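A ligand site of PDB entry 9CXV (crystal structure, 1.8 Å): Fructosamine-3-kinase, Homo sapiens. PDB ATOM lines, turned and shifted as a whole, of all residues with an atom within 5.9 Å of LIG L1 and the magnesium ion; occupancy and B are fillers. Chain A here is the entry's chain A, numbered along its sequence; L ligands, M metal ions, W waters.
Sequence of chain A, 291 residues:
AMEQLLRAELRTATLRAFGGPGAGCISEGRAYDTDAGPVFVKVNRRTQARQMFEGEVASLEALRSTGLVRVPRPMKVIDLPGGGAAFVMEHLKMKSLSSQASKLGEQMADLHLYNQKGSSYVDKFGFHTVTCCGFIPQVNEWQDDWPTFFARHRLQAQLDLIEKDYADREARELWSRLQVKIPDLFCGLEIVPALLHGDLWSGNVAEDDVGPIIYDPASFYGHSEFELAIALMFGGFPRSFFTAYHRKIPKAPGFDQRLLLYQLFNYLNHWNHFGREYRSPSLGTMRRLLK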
ATOM      1  N   CYS A  25     -12.766   8.317 -21.694  1.00  0.00           N
ATOM      2  CA  CYS A  25     -12.830   9.603 -21.002  1.00  0.00           C
ATOM      3  C   CYS A  25     -12.680   9.515 -19.474  1.00  0.00           C
ATOM      4  O   CYS A  25     -12.824   8.440 -18.880  1.00  0.00           O
ATOM      5  CB  CYS A  25     -14.137  10.299 -21.338  1.00  0.00           C
ATOM      6  SG  CYS A  25     -14.338  11.761 -20.322  1.00  0.00           S
ATOM      7  N   ILE A  26     -12.441  10.676 -18.843  1.00  0.00           N
ATOM      8  CA  ILE A  26     -11.887  10.763 -17.486  1.00  0.00           C
ATOM      9  C   ILE A  26     -10.566  10.001 -17.489  1.00  0.00           C
ATOM     10  O   ILE A  26     -10.199   9.380 -16.484  1.00  0.00           O
ATOM     11  CB  ILE A  26     -12.856  10.218 -16.415  1.00  0.00           C
ATOM     12  N   SER A  27      -9.859  10.063 -18.623  1.00  0.00           N
ATOM     13  CA  SER A  27      -8.667   9.255 -18.871  1.00  0.00           C
ATOM     14  C   SER A  27      -8.988   7.747 -18.755  1.00  0.00           C
ATOM     15  O   SER A  27      -8.262   6.972 -18.121  1.00  0.00           O
ATOM     16  CB  SER A  27      -7.519   9.655 -17.943  1.00  0.00           C
ATOM     17  N   GLU A  28     -10.097   7.350 -19.387  1.00  0.00           N
ATOM     18  CA  GLU A  28     -10.379   5.927 -19.601  1.00  0.00           C
ATOM     19  C   GLU A  28      -9.935   5.513 -20.998  1.00  0.00           C
ATOM     20  O   GLU A  28      -8.820   4.993 -21.161  1.00  0.00           O
ATOM     21  CB  GLU A  28     -11.874   5.605 -19.422  1.00  0.00           C
ATOM     22  N   GLY A  29     -10.774   5.765 -22.014  1.00  0.00           N
ATOM     23  CA  GLY A  29     -10.557   5.220 -23.338  1.00  0.00           C
ATOM     24  C   GLY A  29     -11.870   5.201 -24.089  1.00  0.00           C
ATOM     25  O   GLY A  29     -12.690   6.099 -23.876  1.00  0.00           O
ATOM     26  N   ALA A  31     -14.891   2.788 -26.754  1.00  0.00           N
ATOM     27  CA  ALA A  31     -15.577   1.533 -27.058  1.00  0.00           C
ATOM     28  C   ALA A  31     -15.616   1.332 -28.560  1.00  0.00           C
ATOM     29  O   ALA A  31     -15.635   2.305 -29.317  1.00  0.00           O
ATOM     30  CB  ALA A  31     -17.000   1.563 -26.534  1.00  0.00           C
ATOM     31  N   PHE A  40     -15.108  -2.924 -24.882  1.00  0.00           N
ATOM     32  CA  PHE A  40     -14.741  -1.655 -24.329  1.00  0.00           C
ATOM     33  C   PHE A  40     -13.248  -1.686 -24.023  1.00  0.00           C
ATOM     34  O   PHE A  40     -12.759  -2.641 -23.408  1.00  0.00           O
ATOM     35  CB  PHE A  40     -15.583  -1.333 -23.075  1.00  0.00           C
ATOM     36  CG  PHE A  40     -15.317   0.032 -22.556  1.00  0.00           C
ATOM     37  CD1 PHE A  40     -16.019   1.119 -23.068  1.00  0.00           C
ATOM     38  CD2 PHE A  40     -14.356   0.238 -21.596  1.00  0.00           C
ATOM     39  CE1 PHE A  40     -15.749   2.400 -22.603  1.00  0.00           C
ATOM     40  CE2 PHE A  40     -14.090   1.503 -21.114  1.00  0.00           C
ATOM     41  CZ  PHE A  40     -14.783   2.595 -21.614  1.00  0.00           C
ATOM     42  N   LYS A  42      -9.874   0.269 -22.522  1.00  0.00           N
ATOM     43  CA  LYS A  42      -9.284   1.288 -21.665  1.00  0.00           C
ATOM     44  C   LYS A  42      -7.853   1.455 -22.085  1.00  0.00           C
ATOM     45  O   LYS A  42      -7.127   0.473 -22.218  1.00  0.00           O
ATOM     46  CB  LYS A  42      -9.286   0.897 -20.171  1.00  0.00           C
ATOM     47  CG  LYS A  42     -10.577   1.063 -19.401  1.00  0.00           C
ATOM     48  CD  LYS A  42     -10.271   0.934 -17.869  1.00  0.00           C
ATOM     49  CE  LYS A  42     -11.520   0.616 -17.134  1.00  0.00           C
ATOM     50  NZ  LYS A  42     -11.324   0.699 -15.646  1.00  0.00           N
ATOM     51  N   GLU A  56      -6.563  -4.704 -11.894  1.00  0.00           N
ATOM     52  CA  GLU A  56      -7.991  -4.613 -12.187  1.00  0.00           C
ATOM     53  C   GLU A  56      -8.524  -5.927 -12.677  1.00  0.00           C
ATOM     54  O   GLU A  56      -9.648  -6.327 -12.337  1.00  0.00           O
ATOM     55  CB  GLU A  56      -8.280  -3.491 -13.213  1.00  0.00           C
ATOM     56  CG  GLU A  56      -9.777  -3.235 -13.434  1.00  0.00           C
ATOM     57  CD  GLU A  56     -10.049  -2.066 -14.381  1.00  0.00           C
ATOM     58  OE1 GLU A  56      -9.062  -1.374 -14.721  1.00  0.00           O
ATOM     59  OE2 GLU A  56     -11.211  -1.864 -14.804  1.00  0.00           O
ATOM     60  N   PRO A  72     -17.822  -6.541 -15.796  1.00  0.00           N
ATOM     61  CA  PRO A  72     -17.385  -6.831 -17.179  1.00  0.00           C
ATOM     62  C   PRO A  72     -16.300  -7.928 -17.173  1.00  0.00           C
ATOM     63  O   PRO A  72     -15.439  -7.978 -16.302  1.00  0.00           O
ATOM     64  CB  PRO A  72     -16.864  -5.497 -17.693  1.00  0.00           C
ATOM     65  CG  PRO A  72     -16.675  -4.565 -16.536  1.00  0.00           C
ATOM     66  CD  PRO A  72     -17.507  -5.174 -15.349  1.00  0.00           C
ATOM     67  N   MET A  89     -12.170  -5.345 -22.509  1.00  0.00           N
ATOM     68  CA  MET A  89     -13.103  -6.136 -21.719  1.00  0.00           C
ATOM     69  C   MET A  89     -14.451  -6.207 -22.462  1.00  0.00           C
ATOM     70  O   MET A  89     -14.716  -5.414 -23.377  1.00  0.00           O
ATOM     71  CB  MET A  89     -13.403  -5.550 -20.323  1.00  0.00           C
ATOM     72  CG  MET A  89     -14.122  -4.211 -20.307  1.00  0.00           C
ATOM     73  SD  MET A  89     -13.938  -3.430 -18.720  1.00  0.00           S
ATOM     74  CE  MET A  89     -12.351  -2.628 -18.821  1.00  0.00           C
ATOM     75  N   GLU A  90     -15.269  -7.188 -22.083  1.00  0.00           N
ATOM     76  CA  GLU A  90     -16.658  -7.261 -22.551  1.00  0.00           C
ATOM     77  C   GLU A  90     -17.345  -5.908 -22.426  1.00  0.00           C
ATOM     78  O   GLU A  90     -17.190  -5.191 -21.430  1.00  0.00           O
ATOM     79  CB  GLU A  90     -17.403  -8.316 -21.726  1.00  0.00           C
ATOM     80  CG  GLU A  90     -18.938  -8.402 -21.895  1.00  0.00           C
ATOM     81  CD  GLU A  90     -19.565  -9.130 -20.731  1.00  0.00           C
ATOM     82  OE1 GLU A  90     -18.968  -9.078 -19.608  1.00  0.00           O
ATOM     83  OE2 GLU A  90     -20.583  -9.813 -20.933  1.00  0.00           O
ATOM     84  N   HIS A  91     -18.088  -5.520 -23.460  1.00  0.00           N
ATOM     85  CA  HIS A  91     -18.821  -4.280 -23.425  1.00  0.00           C
ATOM     86  C   HIS A  91     -20.211  -4.521 -22.844  1.00  0.00           C
ATOM     87  O   HIS A  91     -20.846  -5.541 -23.134  1.00  0.00           O
ATOM     88  CB  HIS A  91     -18.948  -3.692 -24.825  1.00  0.00           C
ATOM     89  CG  HIS A  91     -19.810  -2.479 -24.888  1.00  0.00           C
ATOM     90  ND1 HIS A  91     -21.182  -2.557 -25.004  1.00  0.00           N
ATOM     91  CD2 HIS A  91     -19.505  -1.168 -24.794  1.00  0.00           C
ATOM     92  CE1 HIS A  91     -21.682  -1.331 -25.021  1.00  0.00           C
ATOM     93  NE2 HIS A  91     -20.680  -0.466 -24.900  1.00  0.00           N
ATOM     94  N   LEU A  92     -20.669  -3.582 -22.025  1.00  0.00           N
ATOM     95  CA  LEU A  92     -21.981  -3.694 -21.366  1.00  0.00           C
ATOM     96  C   LEU A  92     -22.774  -2.419 -21.653  1.00  0.00           C
ATOM     97  O   LEU A  92     -22.282  -1.321 -21.398  1.00  0.00           O
ATOM     98  CB  LEU A  92     -21.806  -3.869 -19.842  1.00  0.00           C
ATOM     99  CG  LEU A  92     -21.205  -5.208 -19.429  1.00  0.00           C
ATOM    100  CD1 LEU A  92     -20.901  -5.169 -17.921  1.00  0.00           C
ATOM    101  CD2 LEU A  92     -22.100  -6.389 -19.792  1.00  0.00           C
ATOM    102  N   LYS A  93     -23.997  -2.558 -22.171  1.00  0.00           N
ATOM    103  CA  LYS A  93     -24.838  -1.366 -22.331  1.00  0.00           C
ATOM    104  C   LYS A  93     -25.312  -0.993 -20.933  1.00  0.00           C
ATOM    105  O   LYS A  93     -25.913  -1.841 -20.259  1.00  0.00           O
ATOM    106  CB  LYS A  93     -26.004  -1.641 -23.275  1.00  0.00           C
ATOM    107  N   MET A  94     -24.992   0.219 -20.479  1.00  0.00           N
ATOM    108  CA  MET A  94     -25.223   0.599 -19.084  1.00  0.00           C
ATOM    109  C   MET A  94     -25.931   1.943 -18.960  1.00  0.00           C
ATOM    110  O   MET A  94     -25.770   2.837 -19.808  1.00  0.00           O
ATOM    111  CB  MET A  94     -23.887   0.718 -18.333  1.00  0.00           C
ATOM    112  CG  MET A  94     -23.142  -0.577 -18.121  1.00  0.00           C
ATOM    113  SD  MET A  94     -21.456  -0.206 -17.492  1.00  0.00           S
ATOM    114  CE  MET A  94     -21.410   1.540 -17.618  1.00  0.00           C
ATOM    115  N   ASP A 199     -13.649   0.396  -4.638  1.00  0.00           N
ATOM    116  CA  ASP A 199     -13.746   1.743  -5.158  1.00  0.00           C
ATOM    117  C   ASP A 199     -15.162   2.041  -5.570  1.00  0.00           C
ATOM    118  O   ASP A 199     -15.452   2.440  -6.713  1.00  0.00           O
ATOM    119  CB  ASP A 199     -12.777   1.908  -6.326  1.00  0.00           C
ATOM    120  CG  ASP A 199     -12.538   3.408  -6.680  1.00  0.00           C
ATOM    121  OD1 ASP A 199     -12.793   4.287  -5.840  1.00  0.00           O
ATOM    122  OD2 ASP A 199     -12.061   3.672  -7.778  1.00  0.00           O
ATOM    123  N   TRP A 201     -17.541   4.081  -5.703  1.00  0.00           N
ATOM    124  CA  TRP A 201     -18.286   5.319  -5.785  1.00  0.00           C
ATOM    125  C   TRP A 201     -19.325   5.247  -6.911  1.00  0.00           C
ATOM    126  O   TRP A 201     -19.358   4.297  -7.710  1.00  0.00           O
ATOM    127  CB  TRP A 201     -17.334   6.495  -5.950  1.00  0.00           C
ATOM    128  CG  TRP A 201     -16.853   6.673  -7.318  1.00  0.00           C
ATOM    129  CD1 TRP A 201     -15.972   5.859  -7.994  1.00  0.00           C
ATOM    130  CD2 TRP A 201     -17.134   7.782  -8.210  1.00  0.00           C
ATOM    131  NE1 TRP A 201     -15.704   6.384  -9.264  1.00  0.00           N
ATOM    132  CE2 TRP A 201     -16.426   7.540  -9.424  1.00  0.00           C
ATOM    133  CE3 TRP A 201     -17.929   8.952  -8.105  1.00  0.00           C
ATOM    134  CZ2 TRP A 201     -16.475   8.435 -10.539  1.00  0.00           C
ATOM    135  CZ3 TRP A 201     -17.972   9.814  -9.212  1.00  0.00           C
ATOM    136  CH2 TRP A 201     -17.251   9.552 -10.392  1.00  0.00           C
ATOM    137  N   GLY A 203     -19.855   6.563  -9.584  1.00  0.00           N
ATOM    138  CA  GLY A 203     -19.489   6.526 -10.992  1.00  0.00           C
ATOM    139  C   GLY A 203     -18.925   5.193 -11.434  1.00  0.00           C
ATOM    140  O   GLY A 203     -18.647   5.009 -12.635  1.00  0.00           O
ATOM    141  N   ASN A 204     -18.748   4.255 -10.495  1.00  0.00           N
ATOM    142  CA  ASN A 204     -18.290   2.892 -10.823  1.00  0.00           C
ATOM    143  C   ASN A 204     -19.401   1.852 -10.712  1.00  0.00           C
ATOM    144  O   ASN A 204     -19.104   0.652 -10.686  1.00  0.00           O
ATOM    145  CB  ASN A 204     -17.118   2.514  -9.918  1.00  0.00           C
ATOM    146  CG  ASN A 204     -15.836   3.196 -10.329  1.00  0.00           C
ATOM    147  OD1 ASN A 204     -15.741   3.666 -11.474  1.00  0.00           O
ATOM    148  ND2 ASN A 204     -14.879   3.271  -9.426  1.00  0.00           N
ATOM    149  N   TYR A 215     -17.986  -1.970 -11.726  1.00  0.00           N
ATOM    150  CA  TYR A 215     -16.783  -2.068 -12.575  1.00  0.00           C
ATOM    151  C   TYR A 215     -15.701  -1.165 -12.000  1.00  0.00           C
ATOM    152  O   TYR A 215     -15.895  -0.523 -10.944  1.00  0.00           O
ATOM    153  CB  TYR A 215     -17.148  -1.702 -14.042  1.00  0.00           C
ATOM    154  CG  TYR A 215     -17.873  -0.377 -14.170  1.00  0.00           C
ATOM    155  CD1 TYR A 215     -17.184   0.824 -14.221  1.00  0.00           C
ATOM    156  CD2 TYR A 215     -19.273  -0.342 -14.208  1.00  0.00           C
ATOM    157  CE1 TYR A 215     -17.859   2.037 -14.280  1.00  0.00           C
ATOM    158  CE2 TYR A 215     -19.962   0.868 -14.266  1.00  0.00           C
ATOM    159  CZ  TYR A 215     -19.241   2.043 -14.320  1.00  0.00           C
ATOM    160  OH  TYR A 215     -19.897   3.258 -14.403  1.00  0.00           O
ATOM    161  N   ASP A 216     -14.503  -1.162 -12.638  1.00  0.00           N
ATOM    162  CA  ASP A 216     -13.340  -0.436 -12.120  1.00  0.00           C
ATOM    163  C   ASP A 216     -13.020  -0.790 -10.652  1.00  0.00           C
ATOM    164  O   ASP A 216     -12.791   0.105  -9.827  1.00  0.00           O
ATOM    165  CB  ASP A 216     -13.624   1.064 -12.209  1.00  0.00           C
ATOM    166  CG  ASP A 216     -12.369   1.895 -12.301  1.00  0.00           C
ATOM    167  OD1 ASP A 216     -11.244   1.330 -12.364  1.00  0.00           O
ATOM    168  OD2 ASP A 216     -12.504   3.135 -12.176  1.00  0.00           O
HETATM  169  P1  LIG L   1     -11.726   4.884 -15.433  1.00  0.00           P
HETATM  170  O1  LIG L   1     -12.562   5.798 -14.554  1.00  0.00           O
HETATM  171  O2  LIG L   1     -10.844   3.879 -14.682  1.00  0.00           O
HETATM  172  O3  LIG L   1     -10.972   5.641 -16.510  1.00  0.00           O
HETATM  173  P2  LIG L   1     -14.095   3.170 -15.720  1.00  0.00           P
HETATM  174  O4  LIG L   1     -13.827   1.664 -15.598  1.00  0.00           O
HETATM  175  O5  LIG L   1     -14.605   3.866 -14.477  1.00  0.00           O
HETATM  176  O6  LIG L   1     -12.796   3.993 -16.275  1.00  0.00           O
HETATM  177  O7  LIG L   1     -15.189   3.438 -16.894  1.00  0.00           O
HETATM  178  C1  LIG L   1     -15.502   4.822 -17.183  1.00  0.00           C
HETATM  179  C2  LIG L   1     -16.756   4.860 -18.051  1.00  0.00           C
HETATM  180  O8  LIG L   1     -16.621   3.960 -19.161  1.00  0.00           O
HETATM  181  C3  LIG L   1     -17.927   4.315 -17.262  1.00  0.00           C
HETATM  182  O9  LIG L   1     -18.533   5.331 -16.457  1.00  0.00           O
HETATM  183  C4  LIG L   1     -18.828   3.707 -18.328  1.00  0.00           C
HETATM  184  O10 LIG L   1     -19.665   4.716 -18.922  1.00  0.00           O
HETATM  185  C5  LIG L   1     -17.833   3.247 -19.387  1.00  0.00           C
HETATM  186  N1  LIG L   1     -17.509   1.802 -19.272  1.00  0.00           N
HETATM  187  C6  LIG L   1     -16.602   1.261 -18.418  1.00  0.00           C
HETATM  188  N2  LIG L   1     -16.512  -0.073 -18.604  1.00  0.00           N
HETATM  189  C7  LIG L   1     -17.413  -0.412 -19.559  1.00  0.00           C
HETATM  190  C8  LIG L   1     -17.839  -1.659 -20.224  1.00  0.00           C
HETATM  191  N3  LIG L   1     -17.285  -2.837 -19.864  1.00  0.00           N
HETATM  192  N4  LIG L   1     -18.780  -1.582 -21.202  1.00  0.00           N
HETATM  193  C9  LIG L   1     -19.299  -0.393 -21.564  1.00  0.00           C
HETATM  194  N5  LIG L   1     -18.967   0.781 -20.986  1.00  0.00           N
HETATM  195  C10 LIG L   1     -18.048   0.829 -20.002  1.00  0.00           C
HETATM  196  N1  LG2 L   2     -13.603  10.496  -7.486  1.00  0.00           N
HETATM  197  C1  LG2 L   2     -13.590   8.986  -7.724  1.00  0.00           C
HETATM  198  C2  LG2 L   2     -12.399   8.294  -8.512  1.00  0.00           C
HETATM  199  O1  LG2 L   2     -11.877   8.802  -9.505  1.00  0.00           O
HETATM  200  C3  LG2 L   2     -13.487  11.291  -8.718  1.00  0.00           C
HETATM  201  C4  LG2 L   2     -13.528  12.840  -8.429  1.00  0.00           C
HETATM  202  C5  LG2 L   2     -14.916  12.432  -6.520  1.00  0.00           C
HETATM  203  C6  LG2 L   2     -14.856  10.905  -6.804  1.00  0.00           C
HETATM  204  C7  LG2 L   2     -11.909   6.841  -8.125  1.00  0.00           C
HETATM  205  C8  LG2 L   2     -10.961   6.852  -6.857  1.00  0.00           C
HETATM  206  C9  LG2 L   2      -9.788   7.935  -6.811  1.00  0.00           C
HETATM  207  C10 LG2 L   2      -8.652   7.902  -7.863  1.00  0.00           C
HETATM  208  O2  LG2 L   2     -14.819  13.194  -7.772  1.00  0.00           O
HETATM  209  O3  LG2 L   2      -9.206   8.032  -9.173  1.00  0.00           O
HETATM  210  O4  LG2 L   2     -10.414   9.225  -6.925  1.00  0.00           O
HETATM  211  O5  LG2 L   2     -11.721   6.809  -5.665  1.00  0.00           O
HETATM  212  O6  LG2 L   2     -11.422   6.086  -9.257  1.00  0.00           O
HETATM  213 MG    MG M   1     -13.996   4.475 -12.805  1.00  0.00          MG
HETATM  214  O   HOH W   1     -13.421   5.826 -11.370  1.00  0.00           O
HETATM  215  O   HOH W   2     -14.614  -0.771 -16.669  1.00  0.00           O
HETATM  216  O   HOH W   3     -16.036   5.656 -13.773  1.00  0.00           O
HETATM  217  O   HOH W   4     -20.609   2.494 -22.423  1.00  0.00           O
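An oxygen (O3) of LIG L1 sits close to the backbone carbonyl oxygen of Ser 27 (3.4 Å).
O of Ile 26 touches O3 of LIG L1, at 3.8 Å.
CZ of Phe 40 touches O8 of LIG L1, 3.4 Å away.
Pro 72 touches LIG L1 (CB to N3, 3.5 Å).
CD2 of His 91 touches C9 of LIG L1, at 3.3 Å.
Met 94 touches LIG L1 (CE to C4, 3.4 Å).
O of Gly 203 touches O9 of LIG L1 (3.8 Å).
Hydrophobic or aromatic side chains within 4 Å of LIG L1: Phe 40, Pro 72, Met 89, His 91, Met 94 and Tyr 215.
Of the 22 residues printed, 15 come within 4 Å of LIG L1.
Water W1 lies within hydrogen-bond range of O6 of LG2 L2, NE1 of Trp 201 and O1 of LIG L1.
Water W2 bridges an oxygen (O4) of LIG L1 (2.8 Å) and the side-chain sulfur of Met 89 (3.4 Å).
The backbone NH (N) of Met 89 is in hydrogen-bond range of the backbone carbonyl oxygen (O) of Phe 40, 2.9 Å away.
N of Tyr 215 lies within hydrogen-bond range of O of Asn 204.
The side-chain amide nitrogen (ND2) of Asn 204 lies within hydrogen-bond range of the backbone carbonyl oxygen (O) of Asp 199, 2.9 Å away.
NZ of Lys 42 is in salt-bridge range of OE2 of Glu 56.
The backbone carbonyl oxygen of Gly 203 sits at hydrogen-bond distance from the side-chain hydroxyl of Tyr 215.
OD1 of Asp 216 lies within salt-bridge range of NZ of Lys 42, at 3.3 Å.
The side-chain amide nitrogen (ND2) of Asn 204 sits close to the indole nitrogen (NE1) of Trp 201, 3.2 Å away.
The magnesium ion is bound by an oxygen (O5) of LIG L1 (1.9 Å), water W1 (2.1 Å), the side-chain carboxylate of Asp 216 (2.1 Å), the side-chain amide oxygen of Asn 204 (2.3 Å) and water W3 (2.5 Å).
Slightly farther from the magnesium ion lies an oxygen (O1) of LIG L1 (2.6 Å).
Two residues have an atom within 4 Å of the magnesium ion: Asn 204 and Asp 216.
Along chain A the residues within 4 Å of the magnesium ion span positions 204 to 216.
The nearest printed residue that does not touch the magnesium ion is Trp 201 (4.4 Å).
SD of Met 89 sits close to N3 of LIG L1, 3.6 Å away.
OH of Tyr 215 lies within hydrogen-bond range of O9 of LIG L1 (3.2 Å).
O3 of LIG L1 sits close to N of Glu 28, at 3.5 Å.
An oxygen (O4) of LIG L1 lies within salt-bridge range of the side-chain amino group (NZ) of Lys 42, at 2.7 Å.
N of Leu 92 is in hydrogen-bond range of N4 of LIG L1 (2.9 Å).
A nitrogen (N3) of LIG L1 sits at hydrogen-bond distance from the backbone carbonyl oxygen (O) of Glu 90 (2.8 Å).
An oxygen (O5) of LG2 L2 lies within hydrogen-bond range of the side-chain carboxylate (OD1) of Asp 199.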
